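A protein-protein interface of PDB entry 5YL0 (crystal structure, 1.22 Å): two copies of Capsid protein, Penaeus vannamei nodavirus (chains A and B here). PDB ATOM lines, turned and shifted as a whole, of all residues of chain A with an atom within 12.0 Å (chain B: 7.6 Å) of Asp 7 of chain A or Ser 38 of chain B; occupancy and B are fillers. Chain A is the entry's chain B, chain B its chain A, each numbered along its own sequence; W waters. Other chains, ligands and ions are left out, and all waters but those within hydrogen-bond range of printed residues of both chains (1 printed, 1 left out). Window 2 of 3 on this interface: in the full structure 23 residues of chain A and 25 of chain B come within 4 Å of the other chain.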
ATOM      1  N   ASP A   7      25.246   5.390  21.623  1.00  0.00           N
ATOM      2  CA  ASP A   7      26.458   6.233  21.576  1.00  0.00           C
ATOM      3  C   ASP A   7      26.115   7.772  21.670  1.00  0.00           C
ATOM      4  O   ASP A   7      25.009   8.177  21.516  1.00  0.00           O
ATOM      5  CB  ASP A   7      27.294   5.814  20.344  1.00  0.00           C
ATOM      6  CG  ASP A   7      28.726   6.140  20.467  1.00  0.00           C
ATOM      7  OD1 ASP A   7      29.213   6.614  21.536  1.00  0.00           O
ATOM      8  OD2 ASP A   7      29.431   5.910  19.434  1.00  0.00           O
ATOM      9  N   VAL A   8      27.121   8.559  21.871  1.00  0.00           N
ATOM     10  CA  VAL A   8      27.059  10.013  22.001  1.00  0.00           C
ATOM     11  C   VAL A   8      28.284  10.631  21.407  1.00  0.00           C
ATOM     12  O   VAL A   8      29.379  10.035  21.398  1.00  0.00           O
ATOM     13  CB  VAL A   8      26.874  10.295  23.486  1.00  0.00           C
ATOM     14  CG1 VAL A   8      28.005   9.884  24.406  1.00  0.00           C
ATOM     15  CG2 VAL A   8      26.427  11.686  23.694  1.00  0.00           C
ATOM     16  N   ARG A   9      28.162  11.872  20.868  1.00  0.00           N
ATOM     17  CA  ARG A   9      29.225  12.500  20.202  1.00  0.00           C
ATOM     18  C   ARG A   9      29.050  14.024  20.247  1.00  0.00           C
ATOM     19  O   ARG A   9      27.929  14.499  20.396  1.00  0.00           O
ATOM     20  CB  ARG A   9      29.281  12.077  18.740  1.00  0.00           C
ATOM     21  CG  ARG A   9      28.064  12.352  17.911  1.00  0.00           C
ATOM     22  CD  ARG A   9      28.238  11.829  16.461  1.00  0.00           C
ATOM     23  NE  ARG A   9      29.561  12.154  15.930  1.00  0.00           N
ATOM     24  CZ  ARG A   9      30.053  13.226  15.264  1.00  0.00           C
ATOM     25  NH1 ARG A   9      29.293  14.252  14.762  1.00  0.00           N
ATOM     26  NH2 ARG A   9      31.388  13.249  15.058  1.00  0.00           N
ATOM     27  N   VAL A  10      30.112  14.731  20.036  1.00  0.00           N
ATOM     28  CA  VAL A  10      30.034  16.181  19.823  1.00  0.00           C
ATOM     29  C   VAL A  10      29.769  16.476  18.339  1.00  0.00           C
ATOM     30  O   VAL A  10      30.589  16.159  17.472  1.00  0.00           O
ATOM     31  CB  VAL A  10      31.306  16.870  20.287  1.00  0.00           C
ATOM     32  CG1 VAL A  10      31.254  18.345  19.964  1.00  0.00           C
ATOM     33  CG2 VAL A  10      31.401  16.734  21.816  1.00  0.00           C
ATOM     34  N   ASP A  11      28.645  17.029  18.051  1.00  0.00           N
ATOM     35  CA  ASP A  11      28.305  17.422  16.706  1.00  0.00           C
ATOM     36  C   ASP A  11      29.082  18.595  16.232  1.00  0.00           C
ATOM     37  O   ASP A  11      29.641  18.559  15.112  1.00  0.00           O
ATOM     38  CB  ASP A  11      26.842  17.646  16.626  1.00  0.00           C
ATOM     39  CG  ASP A  11      26.363  17.839  15.204  1.00  0.00           C
ATOM     40  OD1 ASP A  11      26.276  16.794  14.502  1.00  0.00           O
ATOM     41  OD2 ASP A  11      26.202  19.018  14.767  1.00  0.00           O
ATOM     42  N   THR A  37      15.326  17.124  16.921  1.00  0.00           N
ATOM     43  CA  THR A  37      16.299  16.287  17.593  1.00  0.00           C
ATOM     44  C   THR A  37      16.726  16.908  18.927  1.00  0.00           C
ATOM     45  O   THR A  37      16.779  18.145  19.060  1.00  0.00           O
ATOM     46  CB  THR A  37      17.475  16.059  16.654  1.00  0.00           C
ATOM     47  OG1 THR A  37      16.962  15.376  15.481  1.00  0.00           O
ATOM     48  CG2 THR A  37      18.580  15.227  17.317  1.00  0.00           C
ATOM     49  N   SER A  38      16.914  16.074  19.937  1.00  0.00           N
ATOM     50  CA  SER A  38      17.377  16.510  21.239  1.00  0.00           C
ATOM     51  C   SER A  38      18.895  16.613  21.282  1.00  0.00           C
ATOM     52  O   SER A  38      19.596  15.804  20.779  1.00  0.00           O
ATOM     53  CB  SER A  38      16.920  15.602  22.355  1.00  0.00           C
ATOM     54  OG  SER A  38      15.523  15.549  22.446  1.00  0.00           O
ATOM     55  N   TYR A  39      19.369  17.757  21.886  1.00  0.00           N
ATOM     56  CA  TYR A  39      20.784  17.971  22.082  1.00  0.00           C
ATOM     57  C   TYR A  39      21.043  18.409  23.528  1.00  0.00           C
ATOM     58  O   TYR A  39      20.171  18.889  24.197  1.00  0.00           O
ATOM     59  CB  TYR A  39      21.290  19.074  21.149  1.00  0.00           C
ATOM     60  CG  TYR A  39      21.224  18.696  19.681  1.00  0.00           C
ATOM     61  CD1 TYR A  39      22.214  17.955  19.127  1.00  0.00           C
ATOM     62  CD2 TYR A  39      20.128  18.992  18.858  1.00  0.00           C
ATOM     63  CE1 TYR A  39      22.180  17.581  17.743  1.00  0.00           C
ATOM     64  CE2 TYR A  39      20.067  18.584  17.520  1.00  0.00           C
ATOM     65  CZ  TYR A  39      21.065  17.951  17.011  1.00  0.00           C
ATOM     66  OH  TYR A  39      20.985  17.528  15.637  1.00  0.00           O
ATOM     67  N   LEU A  40      22.297  18.211  23.905  1.00  0.00           N
ATOM     68  CA  LEU A  40      22.790  18.648  25.209  1.00  0.00           C
ATOM     69  C   LEU A  40      23.929  19.621  24.924  1.00  0.00           C
ATOM     70  O   LEU A  40      24.844  19.307  24.155  1.00  0.00           O
ATOM     71  CB  LEU A  40      23.248  17.460  26.037  1.00  0.00           C
ATOM     72  CG  LEU A  40      23.792  17.802  27.394  1.00  0.00           C
ATOM     73  CD1 LEU A  40      22.622  18.149  28.318  1.00  0.00           C
ATOM     74  CD2 LEU A  40      24.562  16.604  28.002  1.00  0.00           C
ATOM     75  N   ILE A 114      27.908  21.049  21.373  1.00  0.00           N
ATOM     76  CA  ILE A 114      26.600  20.527  21.060  1.00  0.00           C
ATOM     77  C   ILE A 114      26.714  19.030  20.951  1.00  0.00           C
ATOM     78  O   ILE A 114      27.388  18.540  20.033  1.00  0.00           O
ATOM     79  CB  ILE A 114      25.998  21.121  19.777  1.00  0.00           C
ATOM     80  CG1 ILE A 114      25.993  22.677  19.830  1.00  0.00           C
ATOM     81  CG2 ILE A 114      24.670  20.575  19.532  1.00  0.00           C
ATOM     82  CD1 ILE A 114      25.424  23.349  18.598  1.00  0.00           C
ATOM     83  N   ILE A 115      26.100  18.303  21.883  1.00  0.00           N
ATOM     84  CA  ILE A 115      26.244  16.858  22.038  1.00  0.00           C
ATOM     85  C   ILE A 115      24.980  16.217  21.586  1.00  0.00           C
ATOM     86  O   ILE A 115      23.907  16.575  21.912  1.00  0.00           O
ATOM     87  CB  ILE A 115      26.599  16.501  23.463  1.00  0.00           C
ATOM     88  CG1 ILE A 115      27.853  17.172  23.891  1.00  0.00           C
ATOM     89  CG2 ILE A 115      26.705  14.960  23.656  1.00  0.00           C
ATOM     90  CD1 ILE A 115      28.014  17.252  25.367  1.00  0.00           C
ATOM     91  N   ALA A 116      25.185  15.128  20.769  1.00  0.00           N
ATOM     92  CA  ALA A 116      24.119  14.393  20.109  1.00  0.00           C
ATOM     93  C   ALA A 116      24.223  12.863  20.370  1.00  0.00           C
ATOM     94  O   ALA A 116      25.281  12.381  20.488  1.00  0.00           O
ATOM     95  CB  ALA A 116      24.200  14.627  18.578  1.00  0.00           C
ATOM     96  N   ALA A 117      23.109  12.205  20.355  1.00  0.00           N
ATOM     97  CA  ALA A 117      23.075  10.738  20.293  1.00  0.00           C
ATOM     98  C   ALA A 117      23.559  10.295  18.894  1.00  0.00           C
ATOM     99  O   ALA A 117      23.342  10.984  17.878  1.00  0.00           O
ATOM    100  CB  ALA A 117      21.691  10.237  20.568  1.00  0.00           C
ATOM    101  N   THR A 118      24.137   9.108  18.833  1.00  0.00           N
ATOM    102  CA  THR A 118      24.436   8.514  17.535  1.00  0.00           C
ATOM    103  C   THR A 118      24.431   6.979  17.748  1.00  0.00           C
ATOM    104  O   THR A 118      24.533   6.439  18.807  1.00  0.00           O
ATOM    105  CB  THR A 118      25.767   9.040  16.989  1.00  0.00           C
ATOM    106  OG1 THR A 118      25.887   8.726  15.608  1.00  0.00           O
ATOM    107  CG2 THR A 118      26.880   8.460  17.715  1.00  0.00           C
ATOM    108  N   VAL B   8      19.515  12.963  25.572  1.00  0.00           N
ATOM    109  CA  VAL B   8      21.001  13.147  25.826  1.00  0.00           C
ATOM    110  C   VAL B   8      21.122  13.895  27.088  1.00  0.00           C
ATOM    111  O   VAL B   8      20.560  14.945  27.226  1.00  0.00           O
ATOM    112  CB  VAL B   8      21.617  13.974  24.683  1.00  0.00           C
ATOM    113  CG1 VAL B   8      23.106  14.019  24.889  1.00  0.00           C
ATOM    114  CG2 VAL B   8      21.207  13.486  23.289  1.00  0.00           C
ATOM    115  N   ASP B  11      24.437  11.972  33.198  1.00  0.00           N
ATOM    116  CA  ASP B  11      24.040  10.931  34.131  1.00  0.00           C
ATOM    117  C   ASP B  11      24.566  11.129  35.518  1.00  0.00           C
ATOM    118  O   ASP B  11      23.945  10.744  36.479  1.00  0.00           O
ATOM    119  CB  ASP B  11      24.436   9.605  33.531  1.00  0.00           C
ATOM    120  CG  ASP B  11      23.375   9.059  32.549  1.00  0.00           C
ATOM    121  OD1 ASP B  11      23.614   7.916  32.110  1.00  0.00           O
ATOM    122  OD2 ASP B  11      22.372   9.768  32.245  1.00  0.00           O
ATOM    123  N   SER B  34      26.744   2.188  33.569  1.00  0.00           N
ATOM    124  CA  SER B  34      26.236   1.014  32.863  1.00  0.00           C
ATOM    125  C   SER B  34      27.344   0.249  32.278  1.00  0.00           C
ATOM    126  O   SER B  34      28.266   0.876  31.755  1.00  0.00           O
ATOM    127  CB  SER B  34      25.297   1.494  31.723  1.00  0.00           C
ATOM    128  OG  SER B  34      24.180   2.098  32.277  1.00  0.00           O
ATOM    129  N   PRO B  35      27.328  -1.099  32.254  1.00  0.00           N
ATOM    130  CA  PRO B  35      28.374  -1.857  31.647  1.00  0.00           C
ATOM    131  C   PRO B  35      28.539  -1.618  30.143  1.00  0.00           C
ATOM    132  O   PRO B  35      27.503  -1.498  29.430  1.00  0.00           O
ATOM    133  CB  PRO B  35      28.003  -3.351  31.963  1.00  0.00           C
ATOM    134  CG  PRO B  35      27.206  -3.276  33.222  1.00  0.00           C
ATOM    135  CD  PRO B  35      26.469  -1.962  33.156  1.00  0.00           C
ATOM    136  N   SER B  36      29.699  -1.660  29.669  1.00  0.00           N
ATOM    137  CA  SER B  36      30.006  -1.677  28.228  1.00  0.00           C
ATOM    138  C   SER B  36      29.275  -0.599  27.474  1.00  0.00           C
ATOM    139  O   SER B  36      28.588  -0.866  26.453  1.00  0.00           O
ATOM    140  CB  SER B  36      29.650  -3.074  27.674  1.00  0.00           C
ATOM    141  OG  SER B  36      30.410  -4.046  28.397  1.00  0.00           O
ATOM    142  N   THR B  37      29.284   0.641  28.005  1.00  0.00           N
ATOM    143  CA  THR B  37      28.521   1.799  27.500  1.00  0.00           C
ATOM    144  C   THR B  37      29.447   2.977  27.238  1.00  0.00           C
ATOM    145  O   THR B  37      30.474   3.135  27.943  1.00  0.00           O
ATOM    146  CB  THR B  37      27.480   2.175  28.495  1.00  0.00           C
ATOM    147  OG1 THR B  37      26.559   1.045  28.644  1.00  0.00           O
ATOM    148  CG2 THR B  37      26.721   3.469  28.153  1.00  0.00           C
ATOM    149  N   SER B  38      29.160   3.695  26.157  1.00  0.00           N
ATOM    150  CA  SER B  38      29.960   4.880  25.759  1.00  0.00           C
ATOM    151  C   SER B  38      29.451   6.139  26.447  1.00  0.00           C
ATOM    152  O   SER B  38      28.307   6.377  26.492  1.00  0.00           O
ATOM    153  CB  SER B  38      29.896   5.082  24.242  1.00  0.00           C
ATOM    154  OG  SER B  38      30.521   4.022  23.555  1.00  0.00           O
ATOM    155  N   TYR B  39      30.409   6.871  26.982  1.00  0.00           N
ATOM    156  CA  TYR B  39      30.175   8.146  27.681  1.00  0.00           C
ATOM    157  C   TYR B  39      31.082   9.191  27.105  1.00  0.00           C
ATOM    158  O   TYR B  39      32.150   8.978  26.579  1.00  0.00           O
ATOM    159  CB  TYR B  39      30.455   7.984  29.183  1.00  0.00           C
ATOM    160  CG  TYR B  39      29.482   7.085  29.894  1.00  0.00           C
ATOM    161  CD1 TYR B  39      28.288   7.531  30.341  1.00  0.00           C
ATOM    162  CD2 TYR B  39      29.760   5.712  30.053  1.00  0.00           C
ATOM    163  CE1 TYR B  39      27.368   6.694  30.998  1.00  0.00           C
ATOM    164  CE2 TYR B  39      28.863   4.864  30.674  1.00  0.00           C
ATOM    165  CZ  TYR B  39      27.684   5.413  31.132  1.00  0.00           C
ATOM    166  OH  TYR B  39      26.714   4.602  31.787  1.00  0.00           O
ATOM    167  N   LEU B  40      30.629  10.421  27.290  1.00  0.00           N
ATOM    168  CA  LEU B  40      31.381  11.623  27.019  1.00  0.00           C
ATOM    169  C   LEU B  40      31.598  12.437  28.284  1.00  0.00           C
ATOM    170  O   LEU B  40      30.627  12.612  29.046  1.00  0.00           O
ATOM    171  CB  LEU B  40      30.624  12.466  25.997  1.00  0.00           C
ATOM    172  CG  LEU B  40      31.284  13.516  25.211  1.00  0.00           C
ATOM    173  CD1 LEU B  40      31.372  14.774  25.996  1.00  0.00           C
ATOM    174  CD2 LEU B  40      32.464  13.048  24.394  1.00  0.00           C
ATOM    175  N   LYS B  86      36.060  10.824  25.295  1.00  0.00           N
ATOM    176  CA  LYS B  86      35.211   9.746  24.951  1.00  0.00           C
ATOM    177  C   LYS B  86      35.787   8.451  25.540  1.00  0.00           C
ATOM    178  O   LYS B  86      36.947   8.109  25.307  1.00  0.00           O
ATOM    179  CB  LYS B  86      35.154   9.594  23.410  1.00  0.00           C
ATOM    180  CG  LYS B  86      34.036   8.780  22.985  1.00  0.00           C
ATOM    181  CD  LYS B  86      32.662   9.438  23.306  1.00  0.00           C
ATOM    182  CE  LYS B  86      31.450   8.543  23.156  1.00  0.00           C
ATOM    183  NZ  LYS B  86      31.448   7.924  21.788  1.00  0.00           N
ATOM    184  N   VAL B  87      34.968   7.770  26.297  1.00  0.00           N
ATOM    185  CA  VAL B  87      35.429   6.571  27.033  1.00  0.00           C
ATOM    186  C   VAL B  87      34.274   5.615  27.118  1.00  0.00           C
ATOM    187  O   VAL B  87      33.145   5.987  27.190  1.00  0.00           O
ATOM    188  CB  VAL B  87      35.957   7.001  28.418  1.00  0.00           C
ATOM    189  CG1 VAL B  87      34.878   7.680  29.220  1.00  0.00           C
ATOM    190  CG2 VAL B  87      36.692   5.887  29.140  1.00  0.00           C
ATOM    191  N   LYS B  88      34.597   4.317  27.143  1.00  0.00           N
ATOM    192  CA  LYS B  88      33.634   3.255  27.339  1.00  0.00           C
ATOM    193  C   LYS B  88      33.903   2.478  28.620  1.00  0.00           C
ATOM    194  O   LYS B  88      35.042   2.207  28.939  1.00  0.00           O
ATOM    195  CB  LYS B  88      33.708   2.286  26.165  1.00  0.00           C
ATOM    196  CG  LYS B  88      32.660   1.242  26.036  1.00  0.00           C
ATOM    197  CD  LYS B  88      32.700   0.598  24.631  1.00  0.00           C
ATOM    198  CE  LYS B  88      31.374  -0.021  24.224  1.00  0.00           C
ATOM    199  NZ  LYS B  88      31.025  -1.287  24.910  1.00  0.00           N
ATOM    200  N   THR B  89      32.813   2.193  29.309  1.00  0.00           N
ATOM    201  CA  THR B  89      32.966   1.385  30.555  1.00  0.00           C
ATOM    202  C   THR B  89      33.245  -0.057  30.224  1.00  0.00           C
ATOM    203  O   THR B  89      32.996  -0.561  29.068  1.00  0.00           O
ATOM    204  CB  THR B  89      31.759   1.429  31.408  1.00  0.00           C
ATOM    205  OG1 THR B  89      30.599   1.151  30.547  1.00  0.00           O
ATOM    206  CG2 THR B  89      31.566   2.752  32.062  1.00  0.00           C
ATOM    207  N   ILE B 114      29.446  13.309  33.220  1.00  0.00           N
ATOM    208  CA  ILE B 114      29.404  12.020  32.556  1.00  0.00           C
ATOM    209  C   ILE B 114      28.167  11.943  31.769  1.00  0.00           C
ATOM    210  O   ILE B 114      27.117  11.861  32.371  1.00  0.00           O
ATOM    211  CB  ILE B 114      29.596  10.879  33.569  1.00  0.00           C
ATOM    212  CG1 ILE B 114      30.808  11.063  34.452  1.00  0.00           C
ATOM    213  CG2 ILE B 114      29.613   9.514  32.862  1.00  0.00           C
ATOM    214  CD1 ILE B 114      30.977  10.011  35.492  1.00  0.00           C
ATOM    215  N   ILE B 115      28.265  11.977  30.446  1.00  0.00           N
ATOM    216  CA  ILE B 115      27.139  12.164  29.553  1.00  0.00           C
ATOM    217  C   ILE B 115      26.888  10.925  28.753  1.00  0.00           C
ATOM    218  O   ILE B 115      27.771  10.332  28.210  1.00  0.00           O
ATOM    219  CB  ILE B 115      27.423  13.366  28.655  1.00  0.00           C
ATOM    220  CG1 ILE B 115      27.422  14.603  29.483  1.00  0.00           C
ATOM    221  CG2 ILE B 115      26.401  13.497  27.521  1.00  0.00           C
ATOM    222  CD1 ILE B 115      28.258  15.734  28.955  1.00  0.00           C
ATOM    223  N   ALA B 116      25.602  10.605  28.608  1.00  0.00           N
ATOM    224  CA  ALA B 116      25.160   9.425  27.881  1.00  0.00           C
ATOM    225  C   ALA B 116      23.893   9.744  27.129  1.00  0.00           C
ATOM    226  O   ALA B 116      23.229  10.670  27.372  1.00  0.00           O
ATOM    227  CB  ALA B 116      24.789   8.302  28.846  1.00  0.00           C
ATOM    228  N   ALA B 117      23.576   8.853  26.158  1.00  0.00           N
ATOM    229  CA  ALA B 117      22.289   8.942  25.427  1.00  0.00           C
ATOM    230  C   ALA B 117      21.508   7.657  25.402  1.00  0.00           C
ATOM    231  O   ALA B 117      20.288   7.855  25.331  1.00  0.00           O
ATOM    232  CB  ALA B 117      22.479   9.479  24.031  1.00  0.00           C
HETATM  233  O   HOH W   1      31.814   4.887  20.133  1.00  0.00           O
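The side-chain amino group (NZ) of Lys 86 of chain B is in hydrogen-bond range of the backbone carbonyl oxygen (O) of Val 8 of chain A (3.0 Å). The side-chain carboxylate (OD1) of Asp 7 of chain A lies within salt-bridge range of the side-chain amino group (NZ) of Lys 86 of chain B, 2.6 Å away.
The backbone NH (N) of Ile 115 of chain A is in hydrogen-bond range of the backbone carbonyl oxygen (O) of Leu 40 of chain A, 2.8 Å away. The backbone NH (N) of Thr 118 of chain A sits at hydrogen-bond distance from the backbone carbonyl oxygen (O) of Asp 7 of chain A (3.0 Å). N of Ile 115 of chain B sits at hydrogen-bond distance from O of Leu 40 of chain B (2.8 Å).
Ser 38 of chain B touches Asp 7 of chain A (CB to OD1, 3.2 Å). Ala 117 of chain B touches Asp 7 of chain A. Val 8 of chain A touches Leu 40 of chain B (CG1 to N, 3.9 Å). Val 8 of chain A touches Ile 115 of chain B (CG1 to O, 3.8 Å). Val 8 of chain B touches Ser 38 of chain A. CB of Leu 40 of chain A touches CG1 of Val 8 of chain B, 3.6 Å away. Leu 40 of chain A touches Ile 115 of chain B. CG2 of Ile 115 of chain A touches CG1 of Val 8 of chain B, at 3.9 Å. CD1 of Ile 115 of chain A touches CD1 of Ile 115 of chain B, at 3.9 Å. Val 8 of chain B touches Ala 117 of chain A (CG2 to N, 3.7 Å).
Asp 7 of chain A touches just these residues of chain B: Ser 38, Lys 86 and Ala 117. Of the printed residues of chain B, Val 8 of chain A touches Leu 40, Lys 86 and Ile 115. Of the printed residues of chain B, Leu 40 of chain A touches Val 8 (3.6 Å) and Ile 115 (3.6 Å). Thr 118 of chain A touches none of the printed residues of chain B. Of the printed residues of chain A, Val 8 of chain B touches Ser 38, Leu 40, Ile 115 and Ala 117. Ser 34 of chain B touches none of the printed residues of chain A. No residue of chain A comes within 4 Å of Thr 37 of chain B. Ser 38 of chain B touches one residue of chain A. Of the printed residues of chain A, Leu 40 of chain B touches Val 8 (3.9 Å). Val 87 of chain B touches none of the printed residues of chain A. No residue of chain A comes within 4 Å of Thr 89 of chain B. No residue of chain A comes within 4 Å of Ala 116 of chain B. Printed residues of chain A within 4 Å of Ala 117 of chain B: Asp 7 and Ala 117. The nearest residue of chain A that does not touch Ser 38 of chain B is Val 8 of chain A (4.1 Å). The nearest printed residue of chain B that does not touch Ala 117 of chain A is Ala 116 of chain B (6.9 Å).
Printed residues of chain A that touch a printed residue of chain B: Asp 7, Val 8, Ser 38, Leu 40, Ile 115 and Ala 117. Hydrophobic or aromatic side chains of chain A within 4 Å of the printed part of chain B: Val 8, Leu 40, Ile 115 and Ala 117. Hydrophobic or aromatic side chains of chain B that line the printed part of chain A: Val 8, Ile 115 and Ala 117. Among the printed residues, 13 pairs touch across the chains. Among the printed residues, Asp or Glu carboxylates within 4 Å of a Lys or Arg side-chain nitrogen of the other chain: Asp 7 of chain A with Lys 86 of chain B.
Val 8 of chain A touches Leu 40 of chain B, and with the chains exchanged Leu 40 of chain A touches Val 8 of chain B. Val 8 of chain A touches Ile 115 of chain B, and with the chains exchanged Ile 115 of chain A touches Val 8 of chain B. Ser 38 of chain A touches Val 8 of chain B, but with the chains exchanged Val 8 of chain A does not touch Ser 38 of chain B (4.1 Å). Ala 117 of chain A touches its own counterpart, Ala 117 of chain B. Positions printed for both chains: 8, 11, 37, 38, 39, 40, 114, 115, 116 and 117.
Water W1 lies within hydrogen-bond range of OD2 of Asp 7 of chain A and NZ of Lys 86 of chain B.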
